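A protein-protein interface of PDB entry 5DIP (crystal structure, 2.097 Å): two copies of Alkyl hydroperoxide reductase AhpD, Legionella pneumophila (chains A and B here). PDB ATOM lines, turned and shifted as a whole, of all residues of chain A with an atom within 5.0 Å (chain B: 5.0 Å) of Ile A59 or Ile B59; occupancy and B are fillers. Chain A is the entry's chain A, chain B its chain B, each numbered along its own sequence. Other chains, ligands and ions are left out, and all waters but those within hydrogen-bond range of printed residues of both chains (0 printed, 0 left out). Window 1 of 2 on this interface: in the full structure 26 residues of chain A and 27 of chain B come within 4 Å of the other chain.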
ATOM      1  N   LEU A  51       6.918  -6.549 -19.368  1.00  0.00           N
ATOM      2  CA  LEU A  51       6.800  -7.079 -20.718  1.00  0.00           C
ATOM      3  C   LEU A  51       5.926  -8.324 -20.645  1.00  0.00           C
ATOM      4  O   LEU A  51       6.109  -9.148 -19.753  1.00  0.00           O
ATOM      5  CB  LEU A  51       8.186  -7.403 -21.306  1.00  0.00           C
ATOM      6  CG  LEU A  51       9.257  -6.303 -21.243  1.00  0.00           C
ATOM      7  CD1 LEU A  51      10.601  -6.814 -21.784  1.00  0.00           C
ATOM      8  CD2 LEU A  51       8.812  -5.063 -22.005  1.00  0.00           C
ATOM      9  N   THR A  55       5.962 -10.968 -25.734  1.00  0.00           N
ATOM     10  CA  THR A  55       7.052 -10.058 -26.033  1.00  0.00           C
ATOM     11  C   THR A  55       8.399 -10.658 -25.603  1.00  0.00           C
ATOM     12  O   THR A  55       9.372 -10.589 -26.342  1.00  0.00           O
ATOM     13  CB  THR A  55       6.822  -8.696 -25.356  1.00  0.00           C
ATOM     14  OG1 THR A  55       5.627  -8.109 -25.881  1.00  0.00           O
ATOM     15  CG2 THR A  55       7.991  -7.762 -25.605  1.00  0.00           C
ATOM     16  N   LYS A  56       8.441 -11.267 -24.417  1.00  0.00           N
ATOM     17  CA  LYS A  56       9.660 -11.918 -23.948  1.00  0.00           C
ATOM     18  C   LYS A  56      10.043 -13.087 -24.861  1.00  0.00           C
ATOM     19  O   LYS A  56      11.218 -13.342 -25.086  1.00  0.00           O
ATOM     20  CB  LYS A  56       9.496 -12.406 -22.505  1.00  0.00           C
ATOM     21  CG  LYS A  56       9.415 -11.289 -21.441  1.00  0.00           C
ATOM     22  CD  LYS A  56       9.252 -11.915 -20.048  1.00  0.00           C
ATOM     23  CE  LYS A  56       9.431 -10.921 -18.919  1.00  0.00           C
ATOM     24  NZ  LYS A  56       8.151 -10.273 -18.592  1.00  0.00           N
ATOM     25  N   GLU A  57       9.055 -13.810 -25.378  1.00  0.00           N
ATOM     26  CA  GLU A  57       9.357 -14.906 -26.296  1.00  0.00           C
ATOM     27  C   GLU A  57       9.835 -14.407 -27.657  1.00  0.00           C
ATOM     28  O   GLU A  57      10.582 -15.095 -28.338  1.00  0.00           O
ATOM     29  CB  GLU A  57       8.145 -15.819 -26.484  1.00  0.00           C
ATOM     30  CG  GLU A  57       7.938 -16.811 -25.344  1.00  0.00           C
ATOM     31  CD  GLU A  57       9.090 -17.795 -25.175  1.00  0.00           C
ATOM     32  OE1 GLU A  57       9.719 -18.213 -26.183  1.00  0.00           O
ATOM     33  OE2 GLU A  57       9.354 -18.164 -24.020  1.00  0.00           O
ATOM     34  N   LEU A  58       9.394 -13.226 -28.062  1.00  0.00           N
ATOM     35  CA  LEU A  58       9.931 -12.621 -29.279  1.00  0.00           C
ATOM     36  C   LEU A  58      11.393 -12.250 -29.043  1.00  0.00           C
ATOM     37  O   LEU A  58      12.243 -12.441 -29.906  1.00  0.00           O
ATOM     38  CB  LEU A  58       9.104 -11.394 -29.679  1.00  0.00           C
ATOM     39  CG  LEU A  58       7.721 -11.717 -30.255  1.00  0.00           C
ATOM     40  CD1 LEU A  58       6.852 -10.456 -30.319  1.00  0.00           C
ATOM     41  CD2 LEU A  58       7.861 -12.351 -31.638  1.00  0.00           C
ATOM     42  N   ILE A  59      11.680 -11.734 -27.853  1.00  0.00           N
ATOM     43  CA  ILE A  59      13.061 -11.454 -27.476  1.00  0.00           C
ATOM     44  C   ILE A  59      13.864 -12.752 -27.525  1.00  0.00           C
ATOM     45  O   ILE A  59      14.960 -12.776 -28.071  1.00  0.00           O
ATOM     46  CB  ILE A  59      13.151 -10.805 -26.079  1.00  0.00           C
ATOM     47  CG1 ILE A  59      12.567  -9.385 -26.121  1.00  0.00           C
ATOM     48  CG2 ILE A  59      14.611 -10.785 -25.572  1.00  0.00           C
ATOM     49  CD1 ILE A  59      12.403  -8.742 -24.730  1.00  0.00           C
ATOM     50  N   ALA A  60      13.296 -13.832 -26.984  1.00  0.00           N
ATOM     51  CA  ALA A  60      13.969 -15.134 -27.002  1.00  0.00           C
ATOM     52  C   ALA A  60      14.237 -15.603 -28.421  1.00  0.00           C
ATOM     53  O   ALA A  60      15.290 -16.169 -28.695  1.00  0.00           O
ATOM     54  CB  ALA A  60      13.148 -16.185 -26.260  1.00  0.00           C
ATOM     55  N   MET A  61      13.281 -15.374 -29.321  1.00  0.00           N
ATOM     56  CA  MET A  61      13.455 -15.813 -30.706  1.00  0.00           C
ATOM     57  C   MET A  61      14.621 -15.084 -31.384  1.00  0.00           C
ATOM     58  O   MET A  61      15.407 -15.696 -32.107  1.00  0.00           O
ATOM     59  CB  MET A  61      12.180 -15.603 -31.525  1.00  0.00           C
ATOM     60  CG  MET A  61      12.395 -15.951 -33.011  1.00  0.00           C
ATOM     61  SD  MET A  61      12.945 -17.674 -33.252  1.00  0.00           S
ATOM     62  CE  MET A  61      11.388 -18.397 -32.896  1.00  0.00           C
ATOM     63  N   ALA A  62      14.707 -13.773 -31.168  1.00  0.00           N
ATOM     64  CA  ALA A  62      15.811 -12.979 -31.702  1.00  0.00           C
ATOM     65  C   ALA A  62      17.152 -13.485 -31.173  1.00  0.00           C
ATOM     66  O   ALA A  62      18.108 -13.617 -31.921  1.00  0.00           O
ATOM     67  CB  ALA A  62      15.636 -11.501 -31.345  1.00  0.00           C
ATOM     68  N   LEU A  63      17.207 -13.747 -29.872  1.00  0.00           N
ATOM     69  CA  LEU A  63      18.402 -14.306 -29.246  1.00  0.00           C
ATOM     70  C   LEU A  63      18.749 -15.679 -29.830  1.00  0.00           C
ATOM     71  O   LEU A  63      19.908 -15.971 -30.084  1.00  0.00           O
ATOM     72  CB  LEU A  63      18.200 -14.404 -27.729  1.00  0.00           C
ATOM     73  CG  LEU A  63      18.206 -13.058 -26.984  1.00  0.00           C
ATOM     74  CD1 LEU A  63      17.775 -13.213 -25.524  1.00  0.00           C
ATOM     75  CD2 LEU A  63      19.574 -12.457 -27.042  1.00  0.00           C
ATOM     76  N   THR A  93      10.768  -9.193 -35.468  1.00  0.00           N
ATOM     77  CA  THR A  93      11.799  -9.648 -34.547  1.00  0.00           C
ATOM     78  C   THR A  93      13.022 -10.170 -35.305  1.00  0.00           C
ATOM     79  O   THR A  93      14.166  -9.870 -34.984  1.00  0.00           O
ATOM     80  CB  THR A  93      11.250 -10.746 -33.642  1.00  0.00           C
ATOM     81  OG1 THR A  93      10.091 -10.249 -32.963  1.00  0.00           O
ATOM     82  CG2 THR A  93      12.291 -11.163 -32.628  1.00  0.00           C
ATOM     83  N   MET A  96      15.211  -7.475 -36.716  1.00  0.00           N
ATOM     84  CA  MET A  96      16.149  -6.913 -35.745  1.00  0.00           C
ATOM     85  C   MET A  96      17.404  -7.773 -35.644  1.00  0.00           C
ATOM     86  O   MET A  96      18.510  -7.247 -35.548  1.00  0.00           O
ATOM     87  CB  MET A  96      15.487  -6.773 -34.363  1.00  0.00           C
ATOM     88  CG  MET A  96      14.463  -5.620 -34.290  1.00  0.00           C
ATOM     89  SD  MET A  96      15.185  -4.019 -34.724  1.00  0.00           S
ATOM     90  CE  MET A  96      16.409  -3.804 -33.435  1.00  0.00           C
ATOM     91  N   LEU B  51       5.484  -4.417 -34.317  1.00  0.00           N
ATOM     92  CA  LEU B  51       6.140  -4.105 -33.039  1.00  0.00           C
ATOM     93  C   LEU B  51       6.464  -2.623 -33.009  1.00  0.00           C
ATOM     94  O   LEU B  51       6.921  -2.079 -34.004  1.00  0.00           O
ATOM     95  CB  LEU B  51       7.429  -4.919 -32.849  1.00  0.00           C
ATOM     96  CG  LEU B  51       7.345  -6.450 -32.928  1.00  0.00           C
ATOM     97  CD1 LEU B  51       8.734  -7.050 -32.712  1.00  0.00           C
ATOM     98  CD2 LEU B  51       6.346  -7.022 -31.921  1.00  0.00           C
ATOM     99  N   THR B  55       9.805  -1.540 -28.346  1.00  0.00           N
ATOM    100  CA  THR B  55       9.899  -2.982 -28.253  1.00  0.00           C
ATOM    101  C   THR B  55      11.084  -3.494 -29.072  1.00  0.00           C
ATOM    102  O   THR B  55      11.843  -4.347 -28.608  1.00  0.00           O
ATOM    103  CB  THR B  55       8.603  -3.656 -28.725  1.00  0.00           C
ATOM    104  OG1 THR B  55       7.513  -3.200 -27.915  1.00  0.00           O
ATOM    105  CG2 THR B  55       8.715  -5.169 -28.639  1.00  0.00           C
ATOM    106  N   LYS B  56      11.258  -2.953 -30.278  1.00  0.00           N
ATOM    107  CA  LYS B  56      12.374  -3.372 -31.117  1.00  0.00           C
ATOM    108  C   LYS B  56      13.706  -2.988 -30.489  1.00  0.00           C
ATOM    109  O   LYS B  56      14.681  -3.724 -30.617  1.00  0.00           O
ATOM    110  CB  LYS B  56      12.263  -2.771 -32.521  1.00  0.00           C
ATOM    111  CG  LYS B  56      11.163  -3.416 -33.355  1.00  0.00           C
ATOM    112  CD  LYS B  56      11.099  -2.781 -34.727  1.00  0.00           C
ATOM    113  CE  LYS B  56       9.950  -3.365 -35.526  1.00  0.00           C
ATOM    114  NZ  LYS B  56      10.037  -2.911 -36.919  1.00  0.00           N
ATOM    115  N   GLU B  57      13.755  -1.842 -29.813  1.00  0.00           N
ATOM    116  CA  GLU B  57      14.999  -1.452 -29.161  1.00  0.00           C
ATOM    117  C   GLU B  57      15.286  -2.296 -27.921  1.00  0.00           C
ATOM    118  O   GLU B  57      16.444  -2.499 -27.578  1.00  0.00           O
ATOM    119  CB  GLU B  57      15.002   0.030 -28.783  1.00  0.00           C
ATOM    120  CG  GLU B  57      15.468   0.937 -29.914  1.00  0.00           C
ATOM    121  CD  GLU B  57      16.894   0.674 -30.398  1.00  0.00           C
ATOM    122  OE1 GLU B  57      17.803   0.385 -29.583  1.00  0.00           O
ATOM    123  OE2 GLU B  57      17.110   0.792 -31.614  1.00  0.00           O
ATOM    124  N   LEU B  58      14.243  -2.781 -27.254  1.00  0.00           N
ATOM    125  CA  LEU B  58      14.439  -3.751 -26.179  1.00  0.00           C
ATOM    126  C   LEU B  58      15.037  -5.048 -26.747  1.00  0.00           C
ATOM    127  O   LEU B  58      15.949  -5.633 -26.169  1.00  0.00           O
ATOM    128  CB  LEU B  58      13.118  -4.017 -25.457  1.00  0.00           C
ATOM    129  CG  LEU B  58      12.662  -2.838 -24.586  1.00  0.00           C
ATOM    130  CD1 LEU B  58      11.196  -2.996 -24.166  1.00  0.00           C
ATOM    131  CD2 LEU B  58      13.565  -2.702 -23.358  1.00  0.00           C
ATOM    132  N   ILE B  59      14.538  -5.476 -27.902  1.00  0.00           N
ATOM    133  CA  ILE B  59      15.116  -6.625 -28.589  1.00  0.00           C
ATOM    134  C   ILE B  59      16.594  -6.345 -28.928  1.00  0.00           C
ATOM    135  O   ILE B  59      17.454  -7.182 -28.681  1.00  0.00           O
ATOM    136  CB  ILE B  59      14.320  -6.975 -29.877  1.00  0.00           C
ATOM    137  CG1 ILE B  59      12.933  -7.511 -29.512  1.00  0.00           C
ATOM    138  CG2 ILE B  59      15.091  -7.993 -30.741  1.00  0.00           C
ATOM    139  CD1 ILE B  59      11.969  -7.580 -30.697  1.00  0.00           C
ATOM    140  N   ALA B  60      16.876  -5.152 -29.454  1.00  0.00           N
ATOM    141  CA  ALA B  60      18.248  -4.750 -29.768  1.00  0.00           C
ATOM    142  C   ALA B  60      19.161  -4.781 -28.537  1.00  0.00           C
ATOM    143  O   ALA B  60      20.316  -5.165 -28.631  1.00  0.00           O
ATOM    144  CB  ALA B  60      18.265  -3.355 -30.383  1.00  0.00           C
ATOM    145  N   MET B  61      18.635  -4.364 -27.388  1.00  0.00           N
ATOM    146  CA  MET B  61      19.424  -4.377 -26.155  1.00  0.00           C
ATOM    147  C   MET B  61      19.786  -5.801 -25.728  1.00  0.00           C
ATOM    148  O   MET B  61      20.931  -6.071 -25.369  1.00  0.00           O
ATOM    149  CB  MET B  61      18.694  -3.690 -25.008  1.00  0.00           C
ATOM    150  CG  MET B  61      19.491  -3.793 -23.702  1.00  0.00           C
ATOM    151  SD  MET B  61      21.163  -3.062 -23.861  1.00  0.00           S
ATOM    152  CE  MET B  61      20.595  -1.404 -23.775  1.00  0.00           C
ATOM    153  N   ALA B  62      18.803  -6.698 -25.753  1.00  0.00           N
ATOM    154  CA  ALA B  62      19.059  -8.106 -25.465  1.00  0.00           C
ATOM    155  C   ALA B  62      20.133  -8.666 -26.416  1.00  0.00           C
ATOM    156  O   ALA B  62      21.029  -9.389 -25.993  1.00  0.00           O
ATOM    157  CB  ALA B  62      17.774  -8.919 -25.579  1.00  0.00           C
ATOM    158  N   LEU B  63      20.028  -8.325 -27.698  1.00  0.00           N
ATOM    159  CA  LEU B  63      21.011  -8.776 -28.690  1.00  0.00           C
ATOM    160  C   LEU B  63      22.393  -8.186 -28.400  1.00  0.00           C
ATOM    161  O   LEU B  63      23.395  -8.871 -28.525  1.00  0.00           O
ATOM    162  CB  LEU B  63      20.563  -8.400 -30.108  1.00  0.00           C
ATOM    163  CG  LEU B  63      19.330  -9.141 -30.640  1.00  0.00           C
ATOM    164  CD1 LEU B  63      18.862  -8.575 -31.976  1.00  0.00           C
ATOM    165  CD2 LEU B  63      19.649 -10.601 -30.796  1.00  0.00           C
ATOM    166  N   THR B  93      14.239  -7.356 -20.086  1.00  0.00           N
ATOM    167  CA  THR B  93      14.888  -7.802 -21.317  1.00  0.00           C
ATOM    168  C   THR B  93      16.287  -8.345 -20.994  1.00  0.00           C
ATOM    169  O   THR B  93      16.702  -9.326 -21.611  1.00  0.00           O
ATOM    170  CB  THR B  93      14.957  -6.701 -22.420  1.00  0.00           C
ATOM    171  OG1 THR B  93      15.266  -7.315 -23.678  1.00  0.00           O
ATOM    172  CG2 THR B  93      15.996  -5.644 -22.124  1.00  0.00           C
ATOM    173  N   MET B  96      15.979 -11.871 -19.936  1.00  0.00           N
ATOM    174  CA  MET B  96      15.910 -12.816 -21.039  1.00  0.00           C
ATOM    175  C   MET B  96      17.302 -13.135 -21.569  1.00  0.00           C
ATOM    176  O   MET B  96      17.585 -14.281 -21.898  1.00  0.00           O
ATOM    177  CB  MET B  96      15.014 -12.281 -22.162  1.00  0.00           C
ATOM    178  CG  MET B  96      13.521 -12.282 -21.794  1.00  0.00           C
ATOM    179  SD  MET B  96      12.892 -13.946 -21.427  1.00  0.00           S
ATOM    180  CE  MET B  96      13.284 -14.804 -22.950  1.00  0.00           C
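Printed residues of chain B within 4 Å of Ile A59: Ile B59 (3.9 Å), Ala B62 (3.7 Å), Thr B93 (3.4 Å) and Met B96 (3.7 Å).
Printed residues of chain A within 4 Å of Ile B59: Ile A59 (3.9 Å), Ala A62 (3.6 Å), Thr A93 (3.97 Å) and Met A96 (3.8 Å).
Of the printed residues of chain A, Thr B93 touches Ile A59.
Of the printed residues of chain B, Leu A63 touches Ala B62 (3.6 Å) and Met B96 (3.8 Å).
Printed residues of chain B within 4 Å of Lys A56: Met B96 (3.3 Å).
Printed residues of chain B within 4 Å of Met A96: Lys B56 (3.3 Å), Ile B59 (3.8 Å), Ala B60 (3.6 Å) and Leu B63 (3.8 Å).
Thr B55 touches none of the printed residues of chain A.
Met B61 touches none of the printed residues of chain A.
The nearest printed residue of chain A that does not touch Ile B59 is Leu A58 (4.9 Å).
The nearest printed residue of chain A that does not touch Lys B56 is Thr A93 (5.9 Å).
NZ of Lys A56 lies within hydrogen-bond range of O of Leu A51 (2.6 Å).
O of Leu B58 lies within hydrogen-bond range of OG1 of Thr B93.
Ile A59 touches Thr B93, and with the chains exchanged Thr A93 touches Ile B59.
Ile A59 touches Met B96, and with the chains exchanged Met A96 touches Ile B59.
Leu A63 touches Met B96, and with the chains exchanged Met A96 touches Leu B63.
Thr A93 touches Leu B51, but with the chains exchanged Leu A51 does not touch Thr B93 (4.1 Å).
12 positions are printed for both chains.
Of the 18 pairs that touch across the chains among the printed residues, 17 have their exchanged pair printed and touching as well.
Printed residues of chain B that touch a printed residue of chain A: Leu B51, Lys B56, Leu B58, Ile B59, Ala B60, Ala B62, Leu B63, Thr B93 and Met B96.
Of the 12 printed residues of chain A, 9 touch a printed residue of chain B.
Among the printed residues, 18 pairs touch across the chains.
Among the printed residues, no Asp or Glu carboxylate lies within 4 Å of a Lys or Arg side-chain nitrogen of the other chain.
Lys A56 touches Met B96 (O to CE, 3.3 Å).
Ile A59 touches Ile B59.
Thr B93 touches Ile A59 (OG1 to CD1, 3.4 Å).
Ile A59 touches Met B96.
Ala A62 touches Ile B59.
Leu A63 touches Met B96.
Leu B51 touches Thr A93.
Met A96 touches Lys B56.
Met A96 touches Ile B59 (CB to CG2, 3.8 Å).
Met A96 touches Leu B63 (O to CD1, 3.8 Å).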
